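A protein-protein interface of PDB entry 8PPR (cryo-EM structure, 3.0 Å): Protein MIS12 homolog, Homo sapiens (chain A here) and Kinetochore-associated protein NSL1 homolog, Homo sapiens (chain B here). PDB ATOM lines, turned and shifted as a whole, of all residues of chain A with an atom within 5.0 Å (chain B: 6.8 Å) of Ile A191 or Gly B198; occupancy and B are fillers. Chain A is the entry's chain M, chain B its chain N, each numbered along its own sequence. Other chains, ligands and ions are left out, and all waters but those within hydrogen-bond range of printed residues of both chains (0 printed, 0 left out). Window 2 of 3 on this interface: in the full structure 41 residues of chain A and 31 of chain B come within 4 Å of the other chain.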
ATOM      1  N   LYS A 187      21.775  20.641 -20.082  1.00  0.00           N
ATOM      2  CA  LYS A 187      22.038  19.746 -21.203  1.00  0.00           C
ATOM      3  C   LYS A 187      22.837  18.528 -20.756  1.00  0.00           C
ATOM      4  O   LYS A 187      22.529  17.388 -21.130  1.00  0.00           O
ATOM      5  CB  LYS A 187      22.782  20.504 -22.300  1.00  0.00           C
ATOM      6  CG  LYS A 187      22.992  19.717 -23.571  1.00  0.00           C
ATOM      7  CD  LYS A 187      23.048  20.653 -24.760  1.00  0.00           C
ATOM      8  CE  LYS A 187      24.183  21.651 -24.606  1.00  0.00           C
ATOM      9  NZ  LYS A 187      24.607  22.217 -25.915  1.00  0.00           N
ATOM     10  N   LEU A 188      23.869  18.754 -19.943  1.00  0.00           N
ATOM     11  CA  LEU A 188      24.685  17.654 -19.450  1.00  0.00           C
ATOM     12  C   LEU A 188      23.897  16.751 -18.516  1.00  0.00           C
ATOM     13  O   LEU A 188      24.132  15.542 -18.489  1.00  0.00           O
ATOM     14  CB  LEU A 188      25.925  18.198 -18.744  1.00  0.00           C
ATOM     15  CG  LEU A 188      26.922  17.144 -18.261  1.00  0.00           C
ATOM     16  CD1 LEU A 188      27.269  16.187 -19.389  1.00  0.00           C
ATOM     17  CD2 LEU A 188      28.174  17.803 -17.713  1.00  0.00           C
ATOM     18  N   GLN A 189      22.970  17.312 -17.742  1.00  0.00           N
ATOM     19  CA  GLN A 189      22.114  16.485 -16.904  1.00  0.00           C
ATOM     20  C   GLN A 189      21.231  15.585 -17.753  1.00  0.00           C
ATOM     21  O   GLN A 189      21.045  14.407 -17.433  1.00  0.00           O
ATOM     22  CB  GLN A 189      21.264  17.365 -15.992  1.00  0.00           C
ATOM     23  CG  GLN A 189      20.687  16.626 -14.801  1.00  0.00           C
ATOM     24  CD  GLN A 189      21.763  16.042 -13.911  1.00  0.00           C
ATOM     25  OE1 GLN A 189      21.930  14.826 -13.836  1.00  0.00           O
ATOM     26  NE2 GLN A 189      22.502  16.911 -13.230  1.00  0.00           N
ATOM     27  N   ASN A 190      20.683  16.124 -18.843  1.00  0.00           N
ATOM     28  CA  ASN A 190      19.899  15.296 -19.756  1.00  0.00           C
ATOM     29  C   ASN A 190      20.755  14.185 -20.349  1.00  0.00           C
ATOM     30  O   ASN A 190      20.325  13.023 -20.432  1.00  0.00           O
ATOM     31  CB  ASN A 190      19.312  16.164 -20.865  1.00  0.00           C
ATOM     32  CG  ASN A 190      18.211  17.071 -20.366  1.00  0.00           C
ATOM     33  OD1 ASN A 190      17.462  16.715 -19.458  1.00  0.00           O
ATOM     34  ND2 ASN A 190      18.113  18.258 -20.952  1.00  0.00           N
ATOM     35  N   ILE A 191      21.975  14.528 -20.763  1.00  0.00           N
ATOM     36  CA  ILE A 191      22.882  13.536 -21.330  1.00  0.00           C
ATOM     37  C   ILE A 191      23.196  12.457 -20.304  1.00  0.00           C
ATOM     38  O   ILE A 191      23.205  11.262 -20.619  1.00  0.00           O
ATOM     39  CB  ILE A 191      24.162  14.225 -21.837  1.00  0.00           C
ATOM     40  CG1 ILE A 191      23.848  15.093 -23.054  1.00  0.00           C
ATOM     41  CG2 ILE A 191      25.224  13.193 -22.175  1.00  0.00           C
ATOM     42  CD1 ILE A 191      25.019  15.924 -23.522  1.00  0.00           C
ATOM     43  N   ARG A 192      23.458  12.864 -19.062  1.00  0.00           N
ATOM     44  CA  ARG A 192      23.769  11.912 -18.003  1.00  0.00           C
ATOM     45  C   ARG A 192      22.582  11.010 -17.713  1.00  0.00           C
ATOM     46  O   ARG A 192      22.756   9.819 -17.443  1.00  0.00           O
ATOM     47  CB  ARG A 192      24.187  12.657 -16.738  1.00  0.00           C
ATOM     48  CG  ARG A 192      25.594  13.208 -16.782  1.00  0.00           C
ATOM     49  CD  ARG A 192      26.148  13.397 -15.384  1.00  0.00           C
ATOM     50  NE  ARG A 192      25.942  12.221 -14.549  1.00  0.00           N
ATOM     51  CZ  ARG A 192      26.342  12.121 -13.289  1.00  0.00           C
ATOM     52  NH1 ARG A 192      26.980  13.111 -12.686  1.00  0.00           N
ATOM     53  NH2 ARG A 192      26.098  10.999 -12.618  1.00  0.00           N
ATOM     54  N   ASP A 193      21.371  11.564 -17.743  1.00  0.00           N
ATOM     55  CA  ASP A 193      20.182  10.748 -17.532  1.00  0.00           C
ATOM     56  C   ASP A 193      20.046   9.698 -18.623  1.00  0.00           C
ATOM     57  O   ASP A 193      19.783   8.523 -18.339  1.00  0.00           O
ATOM     58  CB  ASP A 193      18.945  11.641 -17.490  1.00  0.00           C
ATOM     59  CG  ASP A 193      18.930  12.552 -16.283  1.00  0.00           C
ATOM     60  OD1 ASP A 193      19.796  12.381 -15.399  1.00  0.00           O
ATOM     61  OD2 ASP A 193      18.058  13.443 -16.220  1.00  0.00           O
ATOM     62  N   ASN A 194      20.238  10.105 -19.879  1.00  0.00           N
ATOM     63  CA  ASN A 194      20.172   9.151 -20.983  1.00  0.00           C
ATOM     64  C   ASN A 194      21.237   8.073 -20.820  1.00  0.00           C
ATOM     65  O   ASN A 194      20.967   6.876 -20.993  1.00  0.00           O
ATOM     66  CB  ASN A 194      20.340   9.898 -22.309  1.00  0.00           C
ATOM     67  CG  ASN A 194      20.422   8.971 -23.514  1.00  0.00           C
ATOM     68  OD1 ASN A 194      20.188   7.766 -23.420  1.00  0.00           O
ATOM     69  ND2 ASN A 194      20.766   9.541 -24.662  1.00  0.00           N
ATOM     70  N   VAL A 195      22.457   8.486 -20.471  1.00  0.00           N
ATOM     71  CA  VAL A 195      23.561   7.545 -20.325  1.00  0.00           C
ATOM     72  C   VAL A 195      23.276   6.560 -19.202  1.00  0.00           C
ATOM     73  O   VAL A 195      23.513   5.356 -19.338  1.00  0.00           O
ATOM     74  CB  VAL A 195      24.876   8.309 -20.086  1.00  0.00           C
ATOM     75  CG1 VAL A 195      25.936   7.387 -19.502  1.00  0.00           C
ATOM     76  CG2 VAL A 195      25.362   8.940 -21.380  1.00  0.00           C
ATOM     77  N   GLU A 196      22.768   7.055 -18.074  1.00  0.00           N
ATOM     78  CA  GLU A 196      22.459   6.185 -16.949  1.00  0.00           C
ATOM     79  C   GLU A 196      21.358   5.199 -17.305  1.00  0.00           C
ATOM     80  O   GLU A 196      21.433   4.021 -16.942  1.00  0.00           O
ATOM     81  CB  GLU A 196      22.059   7.020 -15.736  1.00  0.00           C
ATOM     82  CG  GLU A 196      23.236   7.523 -14.930  1.00  0.00           C
ATOM     83  CD  GLU A 196      23.976   6.400 -14.234  1.00  0.00           C
ATOM     84  OE1 GLU A 196      23.333   5.387 -13.890  1.00  0.00           O
ATOM     85  OE2 GLU A 196      25.201   6.530 -14.034  1.00  0.00           O
ATOM     86  N   ALA B 193      33.173  20.823 -23.750  1.00  0.00           N
ATOM     87  CA  ALA B 193      33.970  19.666 -24.137  1.00  0.00           C
ATOM     88  C   ALA B 193      33.418  18.387 -23.523  1.00  0.00           C
ATOM     89  O   ALA B 193      33.292  17.362 -24.204  1.00  0.00           O
ATOM     90  CB  ALA B 193      35.428  19.873 -23.727  1.00  0.00           C
ATOM     91  N   LEU B 194      33.071  18.430 -22.234  1.00  0.00           N
ATOM     92  CA  LEU B 194      32.480  17.258 -21.603  1.00  0.00           C
ATOM     93  C   LEU B 194      31.109  16.945 -22.181  1.00  0.00           C
ATOM     94  O   LEU B 194      30.749  15.771 -22.308  1.00  0.00           O
ATOM     95  CB  LEU B 194      32.381  17.453 -20.092  1.00  0.00           C
ATOM     96  CG  LEU B 194      32.030  16.158 -19.358  1.00  0.00           C
ATOM     97  CD1 LEU B 194      33.012  15.055 -19.722  1.00  0.00           C
ATOM     98  CD2 LEU B 194      31.994  16.369 -17.857  1.00  0.00           C
ATOM     99  N   ILE B 195      30.332  17.971 -22.528  1.00  0.00           N
ATOM    100  CA  ILE B 195      29.040  17.729 -23.162  1.00  0.00           C
ATOM    101  C   ILE B 195      29.231  17.005 -24.488  1.00  0.00           C
ATOM    102  O   ILE B 195      28.507  16.052 -24.805  1.00  0.00           O
ATOM    103  CB  ILE B 195      28.280  19.055 -23.340  1.00  0.00           C
ATOM    104  CG1 ILE B 195      27.738  19.544 -21.997  1.00  0.00           C
ATOM    105  CG2 ILE B 195      27.150  18.897 -24.343  1.00  0.00           C
ATOM    106  CD1 ILE B 195      27.032  20.875 -22.078  1.00  0.00           C
ATOM    107  N   GLU B 196      30.213  17.440 -25.278  1.00  0.00           N
ATOM    108  CA  GLU B 196      30.489  16.787 -26.552  1.00  0.00           C
ATOM    109  C   GLU B 196      30.945  15.349 -26.347  1.00  0.00           C
ATOM    110  O   GLU B 196      30.526  14.443 -27.079  1.00  0.00           O
ATOM    111  CB  GLU B 196      31.545  17.579 -27.320  1.00  0.00           C
ATOM    112  CG  GLU B 196      31.010  18.848 -27.951  1.00  0.00           C
ATOM    113  CD  GLU B 196      29.854  18.587 -28.892  1.00  0.00           C
ATOM    114  OE1 GLU B 196      29.856  17.538 -29.569  1.00  0.00           O
ATOM    115  OE2 GLU B 196      28.935  19.431 -28.948  1.00  0.00           O
ATOM    116  N   GLN B 197      31.810  15.122 -25.356  1.00  0.00           N
ATOM    117  CA  GLN B 197      32.266  13.766 -25.075  1.00  0.00           C
ATOM    118  C   GLN B 197      31.105  12.872 -24.661  1.00  0.00           C
ATOM    119  O   GLN B 197      31.008  11.720 -25.101  1.00  0.00           O
ATOM    120  CB  GLN B 197      33.339  13.790 -23.988  1.00  0.00           C
ATOM    121  CG  GLN B 197      33.586  12.439 -23.342  1.00  0.00           C
ATOM    122  CD  GLN B 197      34.848  12.417 -22.510  1.00  0.00           C
ATOM    123  OE1 GLN B 197      34.819  12.083 -21.326  1.00  0.00           O
ATOM    124  NE2 GLN B 197      35.969  12.775 -23.125  1.00  0.00           N
ATOM    125  N   GLY B 198      30.211  13.388 -23.817  1.00  0.00           N
ATOM    126  CA  GLY B 198      29.053  12.609 -23.415  1.00  0.00           C
ATOM    127  C   GLY B 198      28.123  12.313 -24.573  1.00  0.00           C
ATOM    128  O   GLY B 198      27.558  11.220 -24.663  1.00  0.00           O
ATOM    129  N   GLU B 199      27.945  13.282 -25.472  1.00  0.00           N
ATOM    130  CA  GLU B 199      27.132  13.043 -26.659  1.00  0.00           C
ATOM    131  C   GLU B 199      27.740  11.947 -27.523  1.00  0.00           C
ATOM    132  O   GLU B 199      27.031  11.044 -27.990  1.00  0.00           O
ATOM    133  CB  GLU B 199      26.990  14.335 -27.457  1.00  0.00           C
ATOM    134  CG  GLU B 199      25.784  15.169 -27.079  1.00  0.00           C
ATOM    135  CD  GLU B 199      25.990  16.639 -27.375  1.00  0.00           C
ATOM    136  OE1 GLU B 199      27.119  17.016 -27.754  1.00  0.00           O
ATOM    137  OE2 GLU B 199      25.027  17.420 -27.224  1.00  0.00           O
ATOM    138  N   GLY B 200      29.056  12.002 -27.732  1.00  0.00           N
ATOM    139  CA  GLY B 200      29.717  10.957 -28.494  1.00  0.00           C
ATOM    140  C   GLY B 200      29.591   9.597 -27.839  1.00  0.00           C
ATOM    141  O   GLY B 200      29.400   8.584 -28.516  1.00  0.00           O
ATOM    142  N   PHE B 201      29.694   9.554 -26.512  1.00  0.00           N
ATOM    143  CA  PHE B 201      29.572   8.282 -25.808  1.00  0.00           C
ATOM    144  C   PHE B 201      28.154   7.731 -25.885  1.00  0.00           C
ATOM    145  O   PHE B 201      27.961   6.519 -26.027  1.00  0.00           O
ATOM    146  CB  PHE B 201      30.008   8.441 -24.358  1.00  0.00           C
ATOM    147  CG  PHE B 201      30.035   7.152 -23.607  1.00  0.00           C
ATOM    148  CD1 PHE B 201      30.932   6.159 -23.951  1.00  0.00           C
ATOM    149  CD2 PHE B 201      29.164   6.930 -22.559  1.00  0.00           C
ATOM    150  CE1 PHE B 201      30.956   4.967 -23.267  1.00  0.00           C
ATOM    151  CE2 PHE B 201      29.187   5.742 -21.867  1.00  0.00           C
ATOM    152  CZ  PHE B 201      30.083   4.757 -22.222  1.00  0.00           C
ATOM    153  N   SER B 202      27.149   8.601 -25.787  1.00  0.00           N
ATOM    154  CA  SER B 202      25.773   8.153 -25.972  1.00  0.00           C
ATOM    155  C   SER B 202      25.569   7.619 -27.381  1.00  0.00           C
ATOM    156  O   SER B 202      24.846   6.637 -27.591  1.00  0.00           O
ATOM    157  CB  SER B 202      24.804   9.300 -25.687  1.00  0.00           C
ATOM    158  OG  SER B 202      23.474   8.826 -25.572  1.00  0.00           O
ATOM    159  N   GLN B 203      26.196   8.262 -28.362  1.00  0.00           N
ATOM    160  CA  GLN B 203      26.100   7.788 -29.738  1.00  0.00           C
ATOM    161  C   GLN B 203      26.762   6.418 -29.882  1.00  0.00           C
ATOM    162  O   GLN B 203      26.254   5.533 -30.584  1.00  0.00           O
ATOM    163  CB  GLN B 203      26.738   8.831 -30.653  1.00  0.00           C
ATOM    164  CG  GLN B 203      26.459   8.668 -32.116  1.00  0.00           C
ATOM    165  CD  GLN B 203      26.976   9.833 -32.928  1.00  0.00           C
ATOM    166  OE1 GLN B 203      27.186  10.927 -32.403  1.00  0.00           O
ATOM    167  NE2 GLN B 203      27.182   9.609 -34.219  1.00  0.00           N
ATOM    168  N   VAL B 204      27.889   6.221 -29.197  1.00  0.00           N
ATOM    169  CA  VAL B 204      28.515   4.903 -29.140  1.00  0.00           C
ATOM    170  C   VAL B 204      27.548   3.886 -28.559  1.00  0.00           C
ATOM    171  O   VAL B 204      27.402   2.772 -29.077  1.00  0.00           O
ATOM    172  CB  VAL B 204      29.810   4.964 -28.310  1.00  0.00           C
ATOM    173  CG1 VAL B 204      30.289   3.565 -27.974  1.00  0.00           C
ATOM    174  CG2 VAL B 204      30.869   5.711 -29.055  1.00  0.00           C
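Among the printed residues, merely in contact across the chains: Ile A191 with Glu B199, Ile A191 with Ile B195, Ile A191 with Gly B198, Lys A187 with Ile B195 and Leu A188 with Ile B195.
The side-chain amide nitrogen (ND2) of Asn A194 lies within hydrogen-bond range of the side-chain hydroxyl (OG) of Ser B202 (2.9 Å).
Of the printed residues of chain B, Lys A187 touches Ile B195. Printed residues of chain B within 4 Å of Leu A188: Ile B195. Ile A191 touches just these residues of chain B: Ile B195, Gly B198 and Glu B199. Of the printed residues of chain A, Ile B195 touches Lys A187 (3.9 Å), Leu A188 (3.96 Å) and Ile A191 (3.7 Å). Gly B198 touches just one residue of chain A: Ile A191 (3.9 Å). Of the printed residues of chain A, Glu B199 touches Ile A191 (3.7 Å). Printed residues of chain A within 4 Å of Ser B202: Asn A194 (2.9 Å). The nearest residue of chain B that does not touch Ile A191 is Ser B202 (5.3 Å). The nearest residue of chain A that does not touch Gly B198 is Val A195 (4.6 Å). The nearest printed residue of chain B that does not touch Lys A187 is Glu B199 (4.5 Å).
Hydrophobic or aromatic side chains of chain A within 4 Å of the printed part of chain B: Leu A188 and Ile A191. Of the 12 printed residues of chain B, 4 touch a printed residue of chain A. Printed residues of chain B that touch a printed residue of chain A: Ile B195, Gly B198, Glu B199 and Ser B202. Hydrophobic or aromatic side chains of chain B that line the printed part of chain A: Ile B195. Among the printed residues, 6 pairs touch across the chains. Among the printed residues, no Asp or Glu carboxylate lies within 4 Å of a Lys or Arg side-chain nitrogen of the other chain.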
